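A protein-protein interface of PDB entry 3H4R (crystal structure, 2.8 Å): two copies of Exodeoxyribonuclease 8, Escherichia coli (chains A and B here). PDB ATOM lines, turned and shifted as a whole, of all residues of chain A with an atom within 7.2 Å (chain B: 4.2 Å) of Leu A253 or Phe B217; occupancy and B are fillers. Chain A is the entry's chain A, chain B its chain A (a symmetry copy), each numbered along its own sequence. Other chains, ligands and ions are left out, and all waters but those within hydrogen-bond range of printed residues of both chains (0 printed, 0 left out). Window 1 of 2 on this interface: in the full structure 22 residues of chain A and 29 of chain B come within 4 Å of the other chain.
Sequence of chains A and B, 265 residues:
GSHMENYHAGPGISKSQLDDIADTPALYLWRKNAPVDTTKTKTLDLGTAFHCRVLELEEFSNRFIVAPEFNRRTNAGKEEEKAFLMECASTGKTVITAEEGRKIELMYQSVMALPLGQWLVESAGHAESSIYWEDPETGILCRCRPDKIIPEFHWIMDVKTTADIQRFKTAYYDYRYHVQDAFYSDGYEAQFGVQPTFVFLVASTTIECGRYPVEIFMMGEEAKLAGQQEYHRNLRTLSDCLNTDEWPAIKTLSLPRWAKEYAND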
ATOM      1  N   ASP A  23      -1.335   2.100 -20.141  1.00  0.00           N
ATOM      2  CA  ASP A  23      -0.418   2.800 -19.261  1.00  0.00           C
ATOM      3  C   ASP A  23       0.851   3.062 -20.052  1.00  0.00           C
ATOM      4  O   ASP A  23       1.154   4.206 -20.403  1.00  0.00           O
ATOM      5  CB  ASP A  23      -0.100   1.924 -18.063  1.00  0.00           C
ATOM      6  CG  ASP A  23       0.251   2.729 -16.843  1.00  0.00           C
ATOM      7  OD1 ASP A  23       1.139   3.609 -16.942  1.00  0.00           O
ATOM      8  OD2 ASP A  23      -0.369   2.481 -15.784  1.00  0.00           O
ATOM      9  N   ALA A 249       8.945   2.421 -22.467  1.00  0.00           N
ATOM     10  CA  ALA A 249       8.600   2.267 -21.059  1.00  0.00           C
ATOM     11  C   ALA A 249       8.531   3.604 -20.369  1.00  0.00           C
ATOM     12  O   ALA A 249       7.856   3.768 -19.348  1.00  0.00           O
ATOM     13  CB  ALA A 249       9.631   1.378 -20.352  1.00  0.00           C
ATOM     14  N   ILE A 250       9.234   4.567 -20.943  1.00  0.00           N
ATOM     15  CA  ILE A 250       9.306   5.886 -20.357  1.00  0.00           C
ATOM     16  C   ILE A 250       7.997   6.627 -20.426  1.00  0.00           C
ATOM     17  O   ILE A 250       7.456   6.859 -21.499  1.00  0.00           O
ATOM     18  CB  ILE A 250      10.422   6.718 -21.026  1.00  0.00           C
ATOM     19  CG1 ILE A 250      11.740   5.947 -20.974  1.00  0.00           C
ATOM     20  CG2 ILE A 250      10.621   8.007 -20.285  1.00  0.00           C
ATOM     21  CD1 ILE A 250      12.898   6.679 -21.553  1.00  0.00           C
ATOM     22  N   LYS A 251       7.480   6.974 -19.258  1.00  0.00           N
ATOM     23  CA  LYS A 251       6.237   7.720 -19.159  1.00  0.00           C
ATOM     24  C   LYS A 251       6.654   9.178 -19.000  1.00  0.00           C
ATOM     25  O   LYS A 251       7.196   9.554 -17.956  1.00  0.00           O
ATOM     26  CB  LYS A 251       5.440   7.270 -17.929  1.00  0.00           C
ATOM     27  CG  LYS A 251       4.129   6.540 -18.215  1.00  0.00           C
ATOM     28  CD  LYS A 251       3.009   7.517 -18.575  1.00  0.00           C
ATOM     29  CE  LYS A 251       1.651   6.821 -18.643  1.00  0.00           C
ATOM     30  NZ  LYS A 251       0.538   7.771 -18.924  1.00  0.00           N
ATOM     31  N   THR A 252       6.417   9.990 -20.031  1.00  0.00           N
ATOM     32  CA  THR A 252       6.775  11.401 -19.998  1.00  0.00           C
ATOM     33  C   THR A 252       5.803  12.198 -19.151  1.00  0.00           C
ATOM     34  O   THR A 252       4.604  12.037 -19.275  1.00  0.00           O
ATOM     35  CB  THR A 252       6.791  11.975 -21.399  1.00  0.00           C
ATOM     36  OG1 THR A 252       7.873  11.381 -22.130  1.00  0.00           O
ATOM     37  CG2 THR A 252       6.937  13.491 -21.352  1.00  0.00           C
ATOM     38  N   LEU A 253       6.327  13.069 -18.298  1.00  0.00           N
ATOM     39  CA  LEU A 253       5.491  13.860 -17.404  1.00  0.00           C
ATOM     40  C   LEU A 253       5.267  15.274 -17.868  1.00  0.00           C
ATOM     41  O   LEU A 253       6.100  15.850 -18.563  1.00  0.00           O
ATOM     42  CB  LEU A 253       6.100  13.923 -15.997  1.00  0.00           C
ATOM     43  CG  LEU A 253       6.029  12.706 -15.076  1.00  0.00           C
ATOM     44  CD1 LEU A 253       6.729  13.033 -13.764  1.00  0.00           C
ATOM     45  CD2 LEU A 253       4.569  12.320 -14.834  1.00  0.00           C
ATOM     46  N   SER A 254       4.146  15.843 -17.437  1.00  0.00           N
ATOM     47  CA  SER A 254       3.804  17.205 -17.811  1.00  0.00           C
ATOM     48  C   SER A 254       3.270  17.997 -16.629  1.00  0.00           C
ATOM     49  O   SER A 254       2.479  17.494 -15.835  1.00  0.00           O
ATOM     50  CB  SER A 254       2.759  17.200 -18.935  1.00  0.00           C
ATOM     51  OG  SER A 254       2.736  18.449 -19.608  1.00  0.00           O
ATOM     52  N   LEU A 255       3.709  19.245 -16.530  1.00  0.00           N
ATOM     53  CA  LEU A 255       3.291  20.144 -15.460  1.00  0.00           C
ATOM     54  C   LEU A 255       1.822  19.947 -15.110  1.00  0.00           C
ATOM     55  O   LEU A 255       1.004  19.671 -15.978  1.00  0.00           O
ATOM     56  CB  LEU A 255       3.506  21.599 -15.892  1.00  0.00           C
ATOM     57  CG  LEU A 255       4.937  21.994 -16.254  1.00  0.00           C
ATOM     58  CD1 LEU A 255       4.943  23.315 -16.975  1.00  0.00           C
ATOM     59  CD2 LEU A 255       5.775  22.062 -14.994  1.00  0.00           C
ATOM     60  N   ILE B 165       2.029   5.236  -7.520  1.00  0.00           N
ATOM     61  CA  ILE B 165       2.719   5.554  -8.757  1.00  0.00           C
ATOM     62  C   ILE B 165       1.850   6.542  -9.536  1.00  0.00           C
ATOM     63  O   ILE B 165       2.356   7.426 -10.235  1.00  0.00           O
ATOM     64  CB  ILE B 165       2.967   4.293  -9.580  1.00  0.00           C
ATOM     65  CG1 ILE B 165       3.966   3.423  -8.843  1.00  0.00           C
ATOM     66  CG2 ILE B 165       3.539   4.638 -10.948  1.00  0.00           C
ATOM     67  CD1 ILE B 165       5.256   4.136  -8.593  1.00  0.00           C
ATOM     68  N   PHE B 168       2.245  10.008  -7.960  1.00  0.00           N
ATOM     69  CA  PHE B 168       3.526  10.565  -8.382  1.00  0.00           C
ATOM     70  C   PHE B 168       3.328  11.464  -9.601  1.00  0.00           C
ATOM     71  O   PHE B 168       3.610  12.658  -9.540  1.00  0.00           O
ATOM     72  CB  PHE B 168       4.498   9.434  -8.735  1.00  0.00           C
ATOM     73  CG  PHE B 168       5.889   9.901  -9.063  1.00  0.00           C
ATOM     74  CD1 PHE B 168       6.798  10.178  -8.058  1.00  0.00           C
ATOM     75  CD2 PHE B 168       6.288  10.059 -10.376  1.00  0.00           C
ATOM     76  CE1 PHE B 168       8.077  10.603  -8.356  1.00  0.00           C
ATOM     77  CE2 PHE B 168       7.568  10.484 -10.678  1.00  0.00           C
ATOM     78  CZ  PHE B 168       8.460  10.755  -9.668  1.00  0.00           C
ATOM     79  N   LYS B 169       2.827  10.868 -10.686  1.00  0.00           N
ATOM     80  CA  LYS B 169       2.578  11.534 -11.974  1.00  0.00           C
ATOM     81  C   LYS B 169       2.136  13.005 -11.920  1.00  0.00           C
ATOM     82  O   LYS B 169       2.102  13.689 -12.942  1.00  0.00           O
ATOM     83  CB  LYS B 169       1.560  10.714 -12.779  1.00  0.00           C
ATOM     84  CG  LYS B 169       1.339  11.190 -14.208  1.00  0.00           C
ATOM     85  CD  LYS B 169       0.258  10.368 -14.933  1.00  0.00           C
ATOM     86  CE  LYS B 169       0.699   8.920 -15.216  1.00  0.00           C
ATOM     87  NZ  LYS B 169       1.858   8.799 -16.158  1.00  0.00           N
ATOM     88  N   TYR B 172       5.203  14.746  -8.042  1.00  0.00           N
ATOM     89  CA  TYR B 172       6.580  15.142  -8.248  1.00  0.00           C
ATOM     90  C   TYR B 172       6.760  16.651  -8.165  1.00  0.00           C
ATOM     91  O   TYR B 172       7.647  17.133  -7.468  1.00  0.00           O
ATOM     92  CB  TYR B 172       7.075  14.650  -9.602  1.00  0.00           C
ATOM     93  CG  TYR B 172       6.636  15.506 -10.760  1.00  0.00           C
ATOM     94  CD1 TYR B 172       5.451  15.249 -11.436  1.00  0.00           C
ATOM     95  CD2 TYR B 172       7.404  16.586 -11.171  1.00  0.00           C
ATOM     96  CE1 TYR B 172       5.050  16.050 -12.498  1.00  0.00           C
ATOM     97  CE2 TYR B 172       7.012  17.390 -12.220  1.00  0.00           C
ATOM     98  CZ  TYR B 172       5.840  17.118 -12.878  1.00  0.00           C
ATOM     99  OH  TYR B 172       5.456  17.926 -13.908  1.00  0.00           O
ATOM    100  N   VAL B 199      16.123  10.182 -16.121  1.00  0.00           N
ATOM    101  CA  VAL B 199      15.039   9.245 -15.968  1.00  0.00           C
ATOM    102  C   VAL B 199      14.814   8.876 -14.504  1.00  0.00           C
ATOM    103  O   VAL B 199      15.725   8.409 -13.820  1.00  0.00           O
ATOM    104  CB  VAL B 199      15.342   7.984 -16.796  1.00  0.00           C
ATOM    105  CG1 VAL B 199      14.487   6.861 -16.362  1.00  0.00           C
ATOM    106  CG2 VAL B 199      15.093   8.253 -18.258  1.00  0.00           C
ATOM    107  N   PHE B 200      13.594   9.099 -14.025  1.00  0.00           N
ATOM    108  CA  PHE B 200      13.235   8.755 -12.654  1.00  0.00           C
ATOM    109  C   PHE B 200      12.758   7.317 -12.639  1.00  0.00           C
ATOM    110  O   PHE B 200      11.918   6.935 -13.437  1.00  0.00           O
ATOM    111  CB  PHE B 200      12.106   9.648 -12.152  1.00  0.00           C
ATOM    112  CG  PHE B 200      12.539  11.026 -11.795  1.00  0.00           C
ATOM    113  CD1 PHE B 200      13.030  11.304 -10.529  1.00  0.00           C
ATOM    114  CD2 PHE B 200      12.454  12.055 -12.720  1.00  0.00           C
ATOM    115  CE1 PHE B 200      13.427  12.588 -10.184  1.00  0.00           C
ATOM    116  CE2 PHE B 200      12.849  13.345 -12.386  1.00  0.00           C
ATOM    117  CZ  PHE B 200      13.334  13.613 -11.120  1.00  0.00           C
ATOM    118  N   VAL B 202      10.795   4.986 -10.440  1.00  0.00           N
ATOM    119  CA  VAL B 202       9.960   4.967  -9.252  1.00  0.00           C
ATOM    120  C   VAL B 202       9.459   3.570  -8.959  1.00  0.00           C
ATOM    121  O   VAL B 202       9.134   2.815  -9.871  1.00  0.00           O
ATOM    122  CB  VAL B 202       8.758   5.901  -9.399  1.00  0.00           C
ATOM    123  CG1 VAL B 202       8.032   6.005  -8.080  1.00  0.00           C
ATOM    124  CG2 VAL B 202       9.218   7.271  -9.867  1.00  0.00           C
ATOM    125  N   GLU B 215       7.889   2.090 -12.289  1.00  0.00           N
ATOM    126  CA  GLU B 215       7.634   2.996 -13.404  1.00  0.00           C
ATOM    127  C   GLU B 215       8.825   3.926 -13.672  1.00  0.00           C
ATOM    128  O   GLU B 215       9.328   4.569 -12.751  1.00  0.00           O
ATOM    129  CB  GLU B 215       6.387   3.833 -13.071  1.00  0.00           C
ATOM    130  CG  GLU B 215       5.638   4.412 -14.256  1.00  0.00           C
ATOM    131  CD  GLU B 215       5.145   3.339 -15.209  1.00  0.00           C
ATOM    132  OE1 GLU B 215       5.972   2.836 -16.009  1.00  0.00           O
ATOM    133  OE2 GLU B 215       3.939   2.992 -15.150  1.00  0.00           O
ATOM    134  N   ILE B 216       9.273   3.983 -14.925  1.00  0.00           N
ATOM    135  CA  ILE B 216      10.370   4.869 -15.328  1.00  0.00           C
ATOM    136  C   ILE B 216       9.726   6.151 -15.882  1.00  0.00           C
ATOM    137  O   ILE B 216       9.010   6.114 -16.873  1.00  0.00           O
ATOM    138  CB  ILE B 216      11.250   4.234 -16.431  1.00  0.00           C
ATOM    139  CG1 ILE B 216      12.255   3.259 -15.827  1.00  0.00           C
ATOM    140  CG2 ILE B 216      11.981   5.294 -17.187  1.00  0.00           C
ATOM    141  CD1 ILE B 216      11.691   1.901 -15.547  1.00  0.00           C
ATOM    142  N   PHE B 217       9.968   7.278 -15.226  1.00  0.00           N
ATOM    143  CA  PHE B 217       9.403   8.559 -15.644  1.00  0.00           C
ATOM    144  C   PHE B 217      10.475   9.500 -16.155  1.00  0.00           C
ATOM    145  O   PHE B 217      11.623   9.470 -15.701  1.00  0.00           O
ATOM    146  CB  PHE B 217       8.709   9.260 -14.482  1.00  0.00           C
ATOM    147  CG  PHE B 217       7.467   8.587 -14.013  1.00  0.00           C
ATOM    148  CD1 PHE B 217       6.252   8.838 -14.635  1.00  0.00           C
ATOM    149  CD2 PHE B 217       7.497   7.735 -12.921  1.00  0.00           C
ATOM    150  CE1 PHE B 217       5.082   8.256 -14.171  1.00  0.00           C
ATOM    151  CE2 PHE B 217       6.337   7.148 -12.453  1.00  0.00           C
ATOM    152  CZ  PHE B 217       5.127   7.410 -13.079  1.00  0.00           C
ATOM    153  N   MET B 218      10.086  10.350 -17.092  1.00  0.00           N
ATOM    154  CA  MET B 218      11.001  11.323 -17.654  1.00  0.00           C
ATOM    155  C   MET B 218      10.294  12.651 -17.703  1.00  0.00           C
ATOM    156  O   MET B 218       9.102  12.702 -17.954  1.00  0.00           O
ATOM    157  CB  MET B 218      11.414  10.916 -19.054  1.00  0.00           C
ATOM    158  CG  MET B 218      12.168  11.988 -19.788  1.00  0.00           C
ATOM    159  SD  MET B 218      12.839  11.327 -21.279  1.00  0.00           S
ATOM    160  CE  MET B 218      11.321  11.011 -22.137  1.00  0.00           C
ATOM    161  N   MET B 219      11.021  13.732 -17.471  1.00  0.00           N
ATOM    162  CA  MET B 219      10.375  15.030 -17.484  1.00  0.00           C
ATOM    163  C   MET B 219      10.091  15.586 -18.899  1.00  0.00           C
ATOM    164  O   MET B 219      10.948  15.580 -19.795  1.00  0.00           O
ATOM    165  CB  MET B 219      11.187  16.025 -16.634  1.00  0.00           C
ATOM    166  CG  MET B 219      10.378  16.667 -15.500  1.00  0.00           C
ATOM    167  SD  MET B 219       9.647  15.473 -14.320  1.00  0.00           S
ATOM    168  CE  MET B 219      10.537  15.810 -12.915  1.00  0.00           C
ATOM    169  N   GLY B 220       8.857  16.050 -19.086  1.00  0.00           N
ATOM    170  CA  GLY B 220       8.452  16.604 -20.363  1.00  0.00           C
ATOM    171  C   GLY B 220       9.016  17.989 -20.602  1.00  0.00           C
ATOM    172  O   GLY B 220       9.029  18.832 -19.702  1.00  0.00           O
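O of Met B218 sits at hydrogen-bond distance from N of Leu A253.
NZ of Lys B169 lies close to NZ of Lys A251.
O of Lys A251 is in hydrogen-bond range of N of Met B218 (3.1 Å).
N of Leu A255 is in hydrogen-bond range of OH of Tyr B172.
OD1 of Asp A23 sits close to OE2 of Glu B215, 3.4 Å away.
O of Leu A253 sits at hydrogen-bond distance from N of Gly B220, at 2.8 Å.
The backbone NH (N) of Lys A251 sits at hydrogen-bond distance from the backbone carbonyl oxygen (O) of Ile B216 (3.0 Å).
The backbone NH (N) of Val B202 sits at hydrogen-bond distance from the backbone carbonyl oxygen (O) of Glu B215 (2.8 Å).
The backbone NH (N) of Phe B200 sits at hydrogen-bond distance from the backbone carbonyl oxygen (O) of Phe B217, 2.6 Å away.
OE1 of Glu B215 touches O of Ala A249, at 3.9 Å.
Ala A249 touches Ile B216.
CA of Ile A250 touches O of Ile B216 (3.5 Å).
Lys A251 touches Phe B217 (O to CA, 3.3 Å).
Thr A252 touches Met B218.
Thr A252 touches Gly B220.
Leu A253 touches Lys B169 (CD2 to O, 3.4 Å).
Leu A253 touches Tyr B172 (CD1 to CD1, 3.5 Å).
Leu A253 touches Met B219 (CD1 to SD, 3.8 Å).
OH of Tyr B172 touches C of Ser A254, 3.5 Å away.
Phe B217 touches two residues of chain A.
Of the printed residues of chain B, Asp A23 touches Glu B215 (3.4 Å).
Of the printed residues of chain A, Met B218 touches Ile A250, Lys A251, Thr A252 and Leu A253.
Of the printed residues of chain B, Leu A255 touches Tyr B172 (3.4 Å).
Of the printed residues of chain B, Ile A250 touches Ile B216 and Met B218.
Phe B168 touches none of the printed residues of chain A.
The nearest printed residue of chain B that does not touch Ile A250 is Val B199 (4.3 Å).
Of the 8 printed residues of chain A, 8 touch a printed residue of chain B.
Printed residues of chain A that touch a printed residue of chain B: Asp A23, Ala A249, Ile A250, Lys A251, Thr A252, Leu A253, Ser A254 and Leu A255.
Printed residues of chain B that touch a printed residue of chain A: Lys B169, Tyr B172, Glu B215, Ile B216, Phe B217, Met B218, Met B219 and Gly B220.
Hydrophobic or aromatic side chains of chain B within 4 Å of the printed part of chain A: Tyr B172, Ile B216, Phe B217, Met B218 and Met B219.
No position is printed for both chains.
Of the 19 pairs that touch across the chains among the printed residues, none has its exchanged pair printed and touching as well.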
